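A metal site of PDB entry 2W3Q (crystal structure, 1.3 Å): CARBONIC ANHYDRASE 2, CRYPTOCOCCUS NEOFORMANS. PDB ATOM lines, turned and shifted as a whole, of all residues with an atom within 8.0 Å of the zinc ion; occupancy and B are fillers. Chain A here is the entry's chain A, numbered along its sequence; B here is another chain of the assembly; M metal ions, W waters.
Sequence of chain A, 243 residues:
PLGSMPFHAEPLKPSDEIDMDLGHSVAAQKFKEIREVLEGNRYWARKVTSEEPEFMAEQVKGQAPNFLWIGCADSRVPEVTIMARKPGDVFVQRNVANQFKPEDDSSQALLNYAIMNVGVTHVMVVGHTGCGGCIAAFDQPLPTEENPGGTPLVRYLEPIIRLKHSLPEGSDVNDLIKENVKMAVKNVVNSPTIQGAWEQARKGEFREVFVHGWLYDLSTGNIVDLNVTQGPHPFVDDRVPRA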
ATOM      1  N   GLY A  71      19.091 -29.822  -9.134  1.00  0.00           N
ATOM      2  CA  GLY A  71      17.985 -29.230  -8.419  1.00  0.00           C
ATOM      3  C   GLY A  71      18.408 -28.221  -7.398  1.00  0.00           C
ATOM      4  O   GLY A  71      19.583 -27.919  -7.236  1.00  0.00           O
ATOM      5  N   CYS A  72      17.445 -27.628  -6.710  1.00  0.00           N
ATOM      6  CA  CYS A  72      17.687 -26.628  -5.683  1.00  0.00           C
ATOM      7  C   CYS A  72      17.959 -27.288  -4.332  1.00  0.00           C
ATOM      8  O   CYS A  72      17.430 -28.346  -4.014  1.00  0.00           O
ATOM      9  CB  CYS A  72      16.473 -25.708  -5.559  1.00  0.00           C
ATOM     10  SG  CYS A  72      16.752 -24.222  -4.534  1.00  0.00           S
ATOM     11  N   ALA A  73      18.769 -26.572  -3.556  1.00  0.00           N
ATOM     12  CA  ALA A  73      19.081 -26.889  -2.175  1.00  0.00           C
ATOM     13  C   ALA A  73      17.879 -26.850  -1.247  1.00  0.00           C
ATOM     14  O   ALA A  73      17.979 -27.452  -0.161  1.00  0.00           O
ATOM     15  CB  ALA A  73      20.131 -25.878  -1.698  1.00  0.00           C
ATOM     16  N   ASP A  74      16.832 -26.166  -1.620  1.00  0.00           N
ATOM     17  CA  ASP A  74      15.634 -26.014  -0.810  1.00  0.00           C
ATOM     18  C   ASP A  74      15.231 -27.317  -0.144  1.00  0.00           C
ATOM     19  O   ASP A  74      15.161 -28.365  -0.762  1.00  0.00           O
ATOM     20  CB  ASP A  74      14.501 -25.565  -1.737  1.00  0.00           C
ATOM     21  CG  ASP A  74      13.312 -25.025  -0.976  1.00  0.00           C
ATOM     22  OD1 ASP A  74      12.575 -25.786  -0.324  1.00  0.00           O
ATOM     23  OD2 ASP A  74      13.126 -23.800  -1.053  1.00  0.00           O
ATOM     24  N   SER A  75      15.014 -27.232   1.165  1.00  0.00           N
ATOM     25  CA  SER A  75      14.722 -28.395   1.968  1.00  0.00           C
ATOM     26  C   SER A  75      13.425 -29.081   1.580  1.00  0.00           C
ATOM     27  O   SER A  75      13.167 -30.215   2.009  1.00  0.00           O
ATOM     28  CB  SER A  75      14.686 -27.958   3.446  1.00  0.00           C
ATOM     29  OG  SER A  75      13.614 -27.106   3.724  1.00  0.00           O
ATOM     30  N   ARG A  76      12.577 -28.406   0.809  1.00  0.00           N
ATOM     31  CA  ARG A  76      11.280 -28.988   0.474  1.00  0.00           C
ATOM     32  C   ARG A  76      11.334 -29.803  -0.788  1.00  0.00           C
ATOM     33  O   ARG A  76      10.302 -30.367  -1.188  1.00  0.00           O
ATOM     34  CB  ARG A  76      10.196 -27.912   0.317  1.00  0.00           C
ATOM     35  CG  ARG A  76      10.022 -27.103   1.583  1.00  0.00           C
ATOM     36  CD  ARG A  76       9.237 -25.827   1.363  1.00  0.00           C
ATOM     37  NE  ARG A  76      10.020 -24.869   0.564  1.00  0.00           N
ATOM     38  CZ  ARG A  76       9.597 -23.671   0.160  1.00  0.00           C
ATOM     39  NH1 ARG A  76       8.392 -23.236   0.437  1.00  0.00           N
ATOM     40  NH2 ARG A  76      10.398 -22.890  -0.554  1.00  0.00           N
ATOM     41  N   VAL A  77      12.538 -29.938  -1.379  1.00  0.00           N
ATOM     42  CA  VAL A  77      12.640 -30.680  -2.641  1.00  0.00           C
ATOM     43  C   VAL A  77      13.661 -31.808  -2.627  1.00  0.00           C
ATOM     44  O   VAL A  77      14.597 -31.854  -3.418  1.00  0.00           O
ATOM     45  CB  VAL A  77      12.871 -29.693  -3.828  1.00  0.00           C
ATOM     46  CG1 VAL A  77      12.573 -30.359  -5.148  1.00  0.00           C
ATOM     47  CG2 VAL A  77      11.976 -28.457  -3.704  1.00  0.00           C
ATOM     48  N   ASN A  95      22.106 -27.103  -5.533  1.00  0.00           N
ATOM     49  CA  ASN A  95      22.732 -25.812  -5.249  1.00  0.00           C
ATOM     50  C   ASN A  95      21.625 -24.774  -5.165  1.00  0.00           C
ATOM     51  O   ASN A  95      20.448 -25.126  -5.347  1.00  0.00           O
ATOM     52  CB  ASN A  95      23.810 -25.415  -6.270  1.00  0.00           C
ATOM     53  CG  ASN A  95      23.284 -25.254  -7.676  1.00  0.00           C
ATOM     54  OD1 ASN A  95      22.147 -24.889  -7.906  1.00  0.00           O
ATOM     55  ND2 ASN A  95      24.119 -25.534  -8.659  1.00  0.00           N
ATOM     56  N   VAL A  96      21.954 -23.507  -4.914  1.00  0.00           N
ATOM     57  CA  VAL A  96      20.902 -22.525  -4.734  1.00  0.00           C
ATOM     58  C   VAL A  96      20.302 -22.183  -6.094  1.00  0.00           C
ATOM     59  O   VAL A  96      20.964 -21.762  -7.041  1.00  0.00           O
ATOM     60  CB  VAL A  96      21.427 -21.269  -4.012  1.00  0.00           C
ATOM     61  CG1 VAL A  96      20.359 -20.160  -4.046  1.00  0.00           C
ATOM     62  CG2 VAL A  96      21.873 -21.647  -2.607  1.00  0.00           C
ATOM     63  N   ALA A  97      18.987 -22.386  -6.187  1.00  0.00           N
ATOM     64  CA  ALA A  97      18.216 -22.043  -7.364  1.00  0.00           C
ATOM     65  C   ALA A  97      18.630 -22.816  -8.601  1.00  0.00           C
ATOM     66  O   ALA A  97      18.343 -22.355  -9.711  1.00  0.00           O
ATOM     67  CB  ALA A  97      18.243 -20.556  -7.665  1.00  0.00           C
ATOM     68  N   ASN A  98      19.130 -24.043  -8.430  1.00  0.00           N
ATOM     69  CA  ASN A  98      19.309 -25.009  -9.505  1.00  0.00           C
ATOM     70  C   ASN A  98      19.950 -24.376 -10.761  1.00  0.00           C
ATOM     71  O   ASN A  98      19.475 -24.526 -11.883  1.00  0.00           O
ATOM     72  CB  ASN A  98      18.028 -25.750  -9.900  1.00  0.00           C
ATOM     73  CG  ASN A  98      16.769 -24.959 -10.141  1.00  0.00           C
ATOM     74  OD1 ASN A  98      16.044 -24.662  -9.153  1.00  0.00           O
ATOM     75  ND2 ASN A  98      16.522 -24.490 -11.338  1.00  0.00           N
ATOM     76  N   VAL A 126      15.570 -29.411 -12.423  1.00  0.00           N
ATOM     77  CA  VAL A 126      14.294 -29.345 -11.701  1.00  0.00           C
ATOM     78  C   VAL A 126      14.276 -28.112 -10.826  1.00  0.00           C
ATOM     79  O   VAL A 126      15.010 -28.017  -9.844  1.00  0.00           O
ATOM     80  CB  VAL A 126      14.049 -30.599 -10.837  1.00  0.00           C
ATOM     81  CG1 VAL A 126      12.612 -30.544 -10.328  1.00  0.00           C
ATOM     82  CG2 VAL A 126      14.350 -31.856 -11.626  1.00  0.00           C
ATOM     83  N   GLY A 127      13.413 -27.185 -11.221  1.00  0.00           N
ATOM     84  CA  GLY A 127      13.131 -25.983 -10.423  1.00  0.00           C
ATOM     85  C   GLY A 127      11.890 -26.265  -9.570  1.00  0.00           C
ATOM     86  O   GLY A 127      11.309 -27.350  -9.680  1.00  0.00           O
ATOM     87  N   HIS A 128      11.465 -25.290  -8.776  1.00  0.00           N
ATOM     88  CA  HIS A 128      10.325 -25.528  -7.914  1.00  0.00           C
ATOM     89  C   HIS A 128       9.664 -24.218  -7.543  1.00  0.00           C
ATOM     90  O   HIS A 128      10.319 -23.168  -7.464  1.00  0.00           O
ATOM     91  CB  HIS A 128      10.798 -26.339  -6.667  1.00  0.00           C
ATOM     92  CG  HIS A 128      11.615 -25.496  -5.765  1.00  0.00           C
ATOM     93  ND1 HIS A 128      11.050 -24.758  -4.716  1.00  0.00           N
ATOM     94  CD2 HIS A 128      12.900 -25.155  -5.769  1.00  0.00           C
ATOM     95  CE1 HIS A 128      11.979 -24.060  -4.105  1.00  0.00           C
ATOM     96  NE2 HIS A 128      13.149 -24.274  -4.728  1.00  0.00           N
ATOM     97  N   THR A 129       8.355 -24.283  -7.315  1.00  0.00           N
ATOM     98  CA  THR A 129       7.670 -23.056  -6.872  1.00  0.00           C
ATOM     99  C   THR A 129       8.141 -22.661  -5.478  1.00  0.00           C
ATOM    100  O   THR A 129       8.618 -23.519  -4.716  1.00  0.00           O
ATOM    101  CB  THR A 129       6.143 -23.274  -6.935  1.00  0.00           C
ATOM    102  OG1 THR A 129       5.721 -24.352  -6.102  1.00  0.00           O
ATOM    103  CG2 THR A 129       5.737 -23.591  -8.380  1.00  0.00           C
ATOM    104  N   GLY A 130       8.070 -21.399  -5.123  1.00  0.00           N
ATOM    105  CA  GLY A 130       8.541 -20.931  -3.826  1.00  0.00           C
ATOM    106  C   GLY A 130      10.045 -20.856  -3.755  1.00  0.00           C
ATOM    107  O   GLY A 130      10.584 -20.872  -2.640  1.00  0.00           O
ATOM    108  N   CYS A 131      10.735 -20.784  -4.866  1.00  0.00           N
ATOM    109  CA  CYS A 131      12.204 -20.770  -4.851  1.00  0.00           C
ATOM    110  C   CYS A 131      12.717 -19.434  -4.371  1.00  0.00           C
ATOM    111  O   CYS A 131      12.537 -18.424  -5.009  1.00  0.00           O
ATOM    112  CB  CYS A 131      12.779 -21.105  -6.234  1.00  0.00           C
ATOM    113  SG  CYS A 131      14.577 -21.323  -6.213  1.00  0.00           S
ATOM    114  N   GLY A 132      13.391 -19.453  -3.222  1.00  0.00           N
ATOM    115  CA  GLY A 132      13.877 -18.237  -2.619  1.00  0.00           C
ATOM    116  C   GLY A 132      14.854 -17.450  -3.438  1.00  0.00           C
ATOM    117  O   GLY A 132      14.778 -16.235  -3.423  1.00  0.00           O
ATOM    118  N   GLY A 133      15.753 -18.116  -4.169  1.00  0.00           N
ATOM    119  CA  GLY A 133      16.686 -17.365  -4.986  1.00  0.00           C
ATOM    120  C   GLY A 133      15.990 -16.630  -6.098  1.00  0.00           C
ATOM    121  O   GLY A 133      16.328 -15.474  -6.408  1.00  0.00           O
ATOM    122  N   CYS A 134      15.005 -17.333  -6.690  1.00  0.00           N
ATOM    123  CA  CYS A 134      14.226 -16.675  -7.739  1.00  0.00           C
ATOM    124  C   CYS A 134      13.359 -15.554  -7.178  1.00  0.00           C
ATOM    125  O   CYS A 134      13.246 -14.522  -7.777  1.00  0.00           O
ATOM    126  CB  CYS A 134      13.406 -17.712  -8.468  1.00  0.00           C
ATOM    127  SG  CYS A 134      14.422 -18.877  -9.441  1.00  0.00           S
ATOM    128  N   ILE A 135      12.719 -15.735  -6.037  1.00  0.00           N
ATOM    129  CA  ILE A 135      11.919 -14.692  -5.407  1.00  0.00           C
ATOM    130  C   ILE A 135      12.793 -13.492  -5.120  1.00  0.00           C
ATOM    131  O   ILE A 135      12.412 -12.343  -5.341  1.00  0.00           O
ATOM    132  CB  ILE A 135      11.224 -15.246  -4.140  1.00  0.00           C
ATOM    133  CG1 ILE A 135      10.129 -16.273  -4.483  1.00  0.00           C
ATOM    134  CG2 ILE A 135      10.636 -14.162  -3.295  1.00  0.00           C
ATOM    135  CD1 ILE A 135       9.671 -17.061  -3.280  1.00  0.00           C
ATOM    136  N   ILE A 177      10.817 -18.629 -12.466  1.00  0.00           N
ATOM    137  CA  ILE A 177      11.309 -19.923 -12.025  1.00  0.00           C
ATOM    138  C   ILE A 177      11.383 -20.869 -13.210  1.00  0.00           C
ATOM    139  O   ILE A 177      12.370 -21.577 -13.424  1.00  0.00           O
ATOM    140  CB  ILE A 177      10.404 -20.432 -10.896  1.00  0.00           C
ATOM    141  CG1 ILE A 177      10.567 -19.566  -9.645  1.00  0.00           C
ATOM    142  CG2 ILE A 177      10.645 -21.906 -10.550  1.00  0.00           C
ATOM    143  CD1 ILE A 177       9.606 -19.903  -8.540  1.00  0.00           C
ATOM    144  N   ASN A 180      14.109 -19.857 -15.527  1.00  0.00           N
ATOM    145  CA  ASN A 180      15.414 -20.201 -14.907  1.00  0.00           C
ATOM    146  C   ASN A 180      15.722 -21.652 -15.157  1.00  0.00           C
ATOM    147  O   ASN A 180      16.870 -22.019 -15.458  1.00  0.00           O
ATOM    148  CB  ASN A 180      15.387 -19.880 -13.438  1.00  0.00           C
ATOM    149  CG  ASN A 180      16.679 -20.167 -12.711  1.00  0.00           C
ATOM    150  OD1 ASN A 180      17.688 -19.629 -13.143  1.00  0.00           O
ATOM    151  ND2 ASN A 180      16.632 -20.986 -11.658  1.00  0.00           N
ATOM    152  N   LEU A 218       4.996 -27.131  -5.499  1.00  0.00           N
ATOM    153  CA  LEU A 218       4.839 -27.437  -4.068  1.00  0.00           C
ATOM    154  C   LEU A 218       3.366 -27.474  -3.681  1.00  0.00           C
ATOM    155  O   LEU A 218       3.062 -28.124  -2.677  1.00  0.00           O
ATOM    156  CB  LEU A 218       5.541 -26.433  -3.178  1.00  0.00           C
ATOM    157  CG  LEU A 218       7.023 -26.652  -2.894  1.00  0.00           C
ATOM    158  CD1 LEU A 218       7.872 -26.774  -4.149  1.00  0.00           C
ATOM    159  CD2 LEU A 218       7.558 -25.517  -2.016  1.00  0.00           C
ATOM    160  N   GLN B  63      10.065 -22.394   4.477  1.00  0.00           N
ATOM    161  CA  GLN B  63      10.963 -23.422   4.988  1.00  0.00           C
ATOM    162  C   GLN B  63      11.789 -22.813   6.111  1.00  0.00           C
ATOM    163  O   GLN B  63      12.181 -21.654   6.085  1.00  0.00           O
ATOM    164  CB  GLN B  63      11.847 -24.023   3.897  1.00  0.00           C
ATOM    165  CG  GLN B  63      12.847 -23.042   3.351  1.00  0.00           C
ATOM    166  CD  GLN B  63      14.056 -23.609   2.667  1.00  0.00           C
ATOM    167  OE1 GLN B  63      14.433 -24.790   2.721  1.00  0.00           O
ATOM    168  NE2 GLN B  63      14.793 -22.751   1.955  1.00  0.00           N
ATOM    169  N   PHE B  91      18.286 -28.578   4.401  1.00  0.00           N
ATOM    170  CA  PHE B  91      18.797 -27.807   3.279  1.00  0.00           C
ATOM    171  C   PHE B  91      20.030 -28.543   2.757  1.00  0.00           C
ATOM    172  O   PHE B  91      20.781 -29.071   3.542  1.00  0.00           O
ATOM    173  CB  PHE B  91      19.169 -26.392   3.749  1.00  0.00           C
ATOM    174  CG  PHE B  91      19.280 -25.324   2.696  1.00  0.00           C
ATOM    175  CD1 PHE B  91      18.180 -24.922   1.973  1.00  0.00           C
ATOM    176  CD2 PHE B  91      20.504 -24.708   2.426  1.00  0.00           C
ATOM    177  CE1 PHE B  91      18.308 -23.922   1.019  1.00  0.00           C
ATOM    178  CE2 PHE B  91      20.639 -23.713   1.477  1.00  0.00           C
ATOM    179  CZ  PHE B  91      19.533 -23.335   0.753  1.00  0.00           C
ATOM    180  N   TYR B 113      24.011 -18.076   2.520  1.00  0.00           N
ATOM    181  CA  TYR B 113      22.564 -18.031   2.449  1.00  0.00           C
ATOM    182  C   TYR B 113      21.937 -18.951   3.482  1.00  0.00           C
ATOM    183  O   TYR B 113      20.974 -18.583   4.138  1.00  0.00           O
ATOM    184  CB  TYR B 113      22.138 -18.445   1.073  1.00  0.00           C
ATOM    185  CG  TYR B 113      20.715 -18.361   0.637  1.00  0.00           C
ATOM    186  CD1 TYR B 113      19.936 -17.235   0.668  1.00  0.00           C
ATOM    187  CD2 TYR B 113      20.124 -19.498   0.110  1.00  0.00           C
ATOM    188  CE1 TYR B 113      18.637 -17.233   0.239  1.00  0.00           C
ATOM    189  CE2 TYR B 113      18.821 -19.487  -0.346  1.00  0.00           C
ATOM    190  CZ  TYR B 113      18.065 -18.359  -0.279  1.00  0.00           C
ATOM    191  OH  TYR B 113      16.763 -18.289  -0.727  1.00  0.00           O
HETATM  192 ZN    ZN M   1      14.823 -23.047  -4.673  1.00  0.00          ZN
HETATM  193  O   HOH W   1      14.380 -22.307  -2.796  1.00  0.00           O
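The side-chain carboxylate (OD1) of Asp 74 is in salt-bridge range of the guanidinium group (NE) of Arg 76, at 2.9 Å. The backbone NH (N) of Asp 74 lies close to the side-chain sulfur (SG) of Cys 72, at 3.5 Å. The side-chain sulfur of Cys 72 lies close to the backbone NH of Ala 97, 3.3 Å away.
CB of Asp 74 touches the zinc ion, at 3.9 Å. Four residues have an atom within 4 Å of the zinc ion: Cys 72, Asp 74, His 128 and Cys 131. The nearest printed residue that does not touch the zinc ion is Gly 132 (4.1 Å).
The zinc ion is bound by water W1 (2.1 Å), NE2 of His 128 (2.1 Å), SG of Cys 72 (2.3 Å) and SG of Cys 131 (2.3 Å). The zinc ion has four donor atoms within binding distance.
Water W1 bridges the side-chain carboxylate (OD2) of Asp 74 (2.6 Å) and the backbone NH (N) of Gly 132 (3.1 Å).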
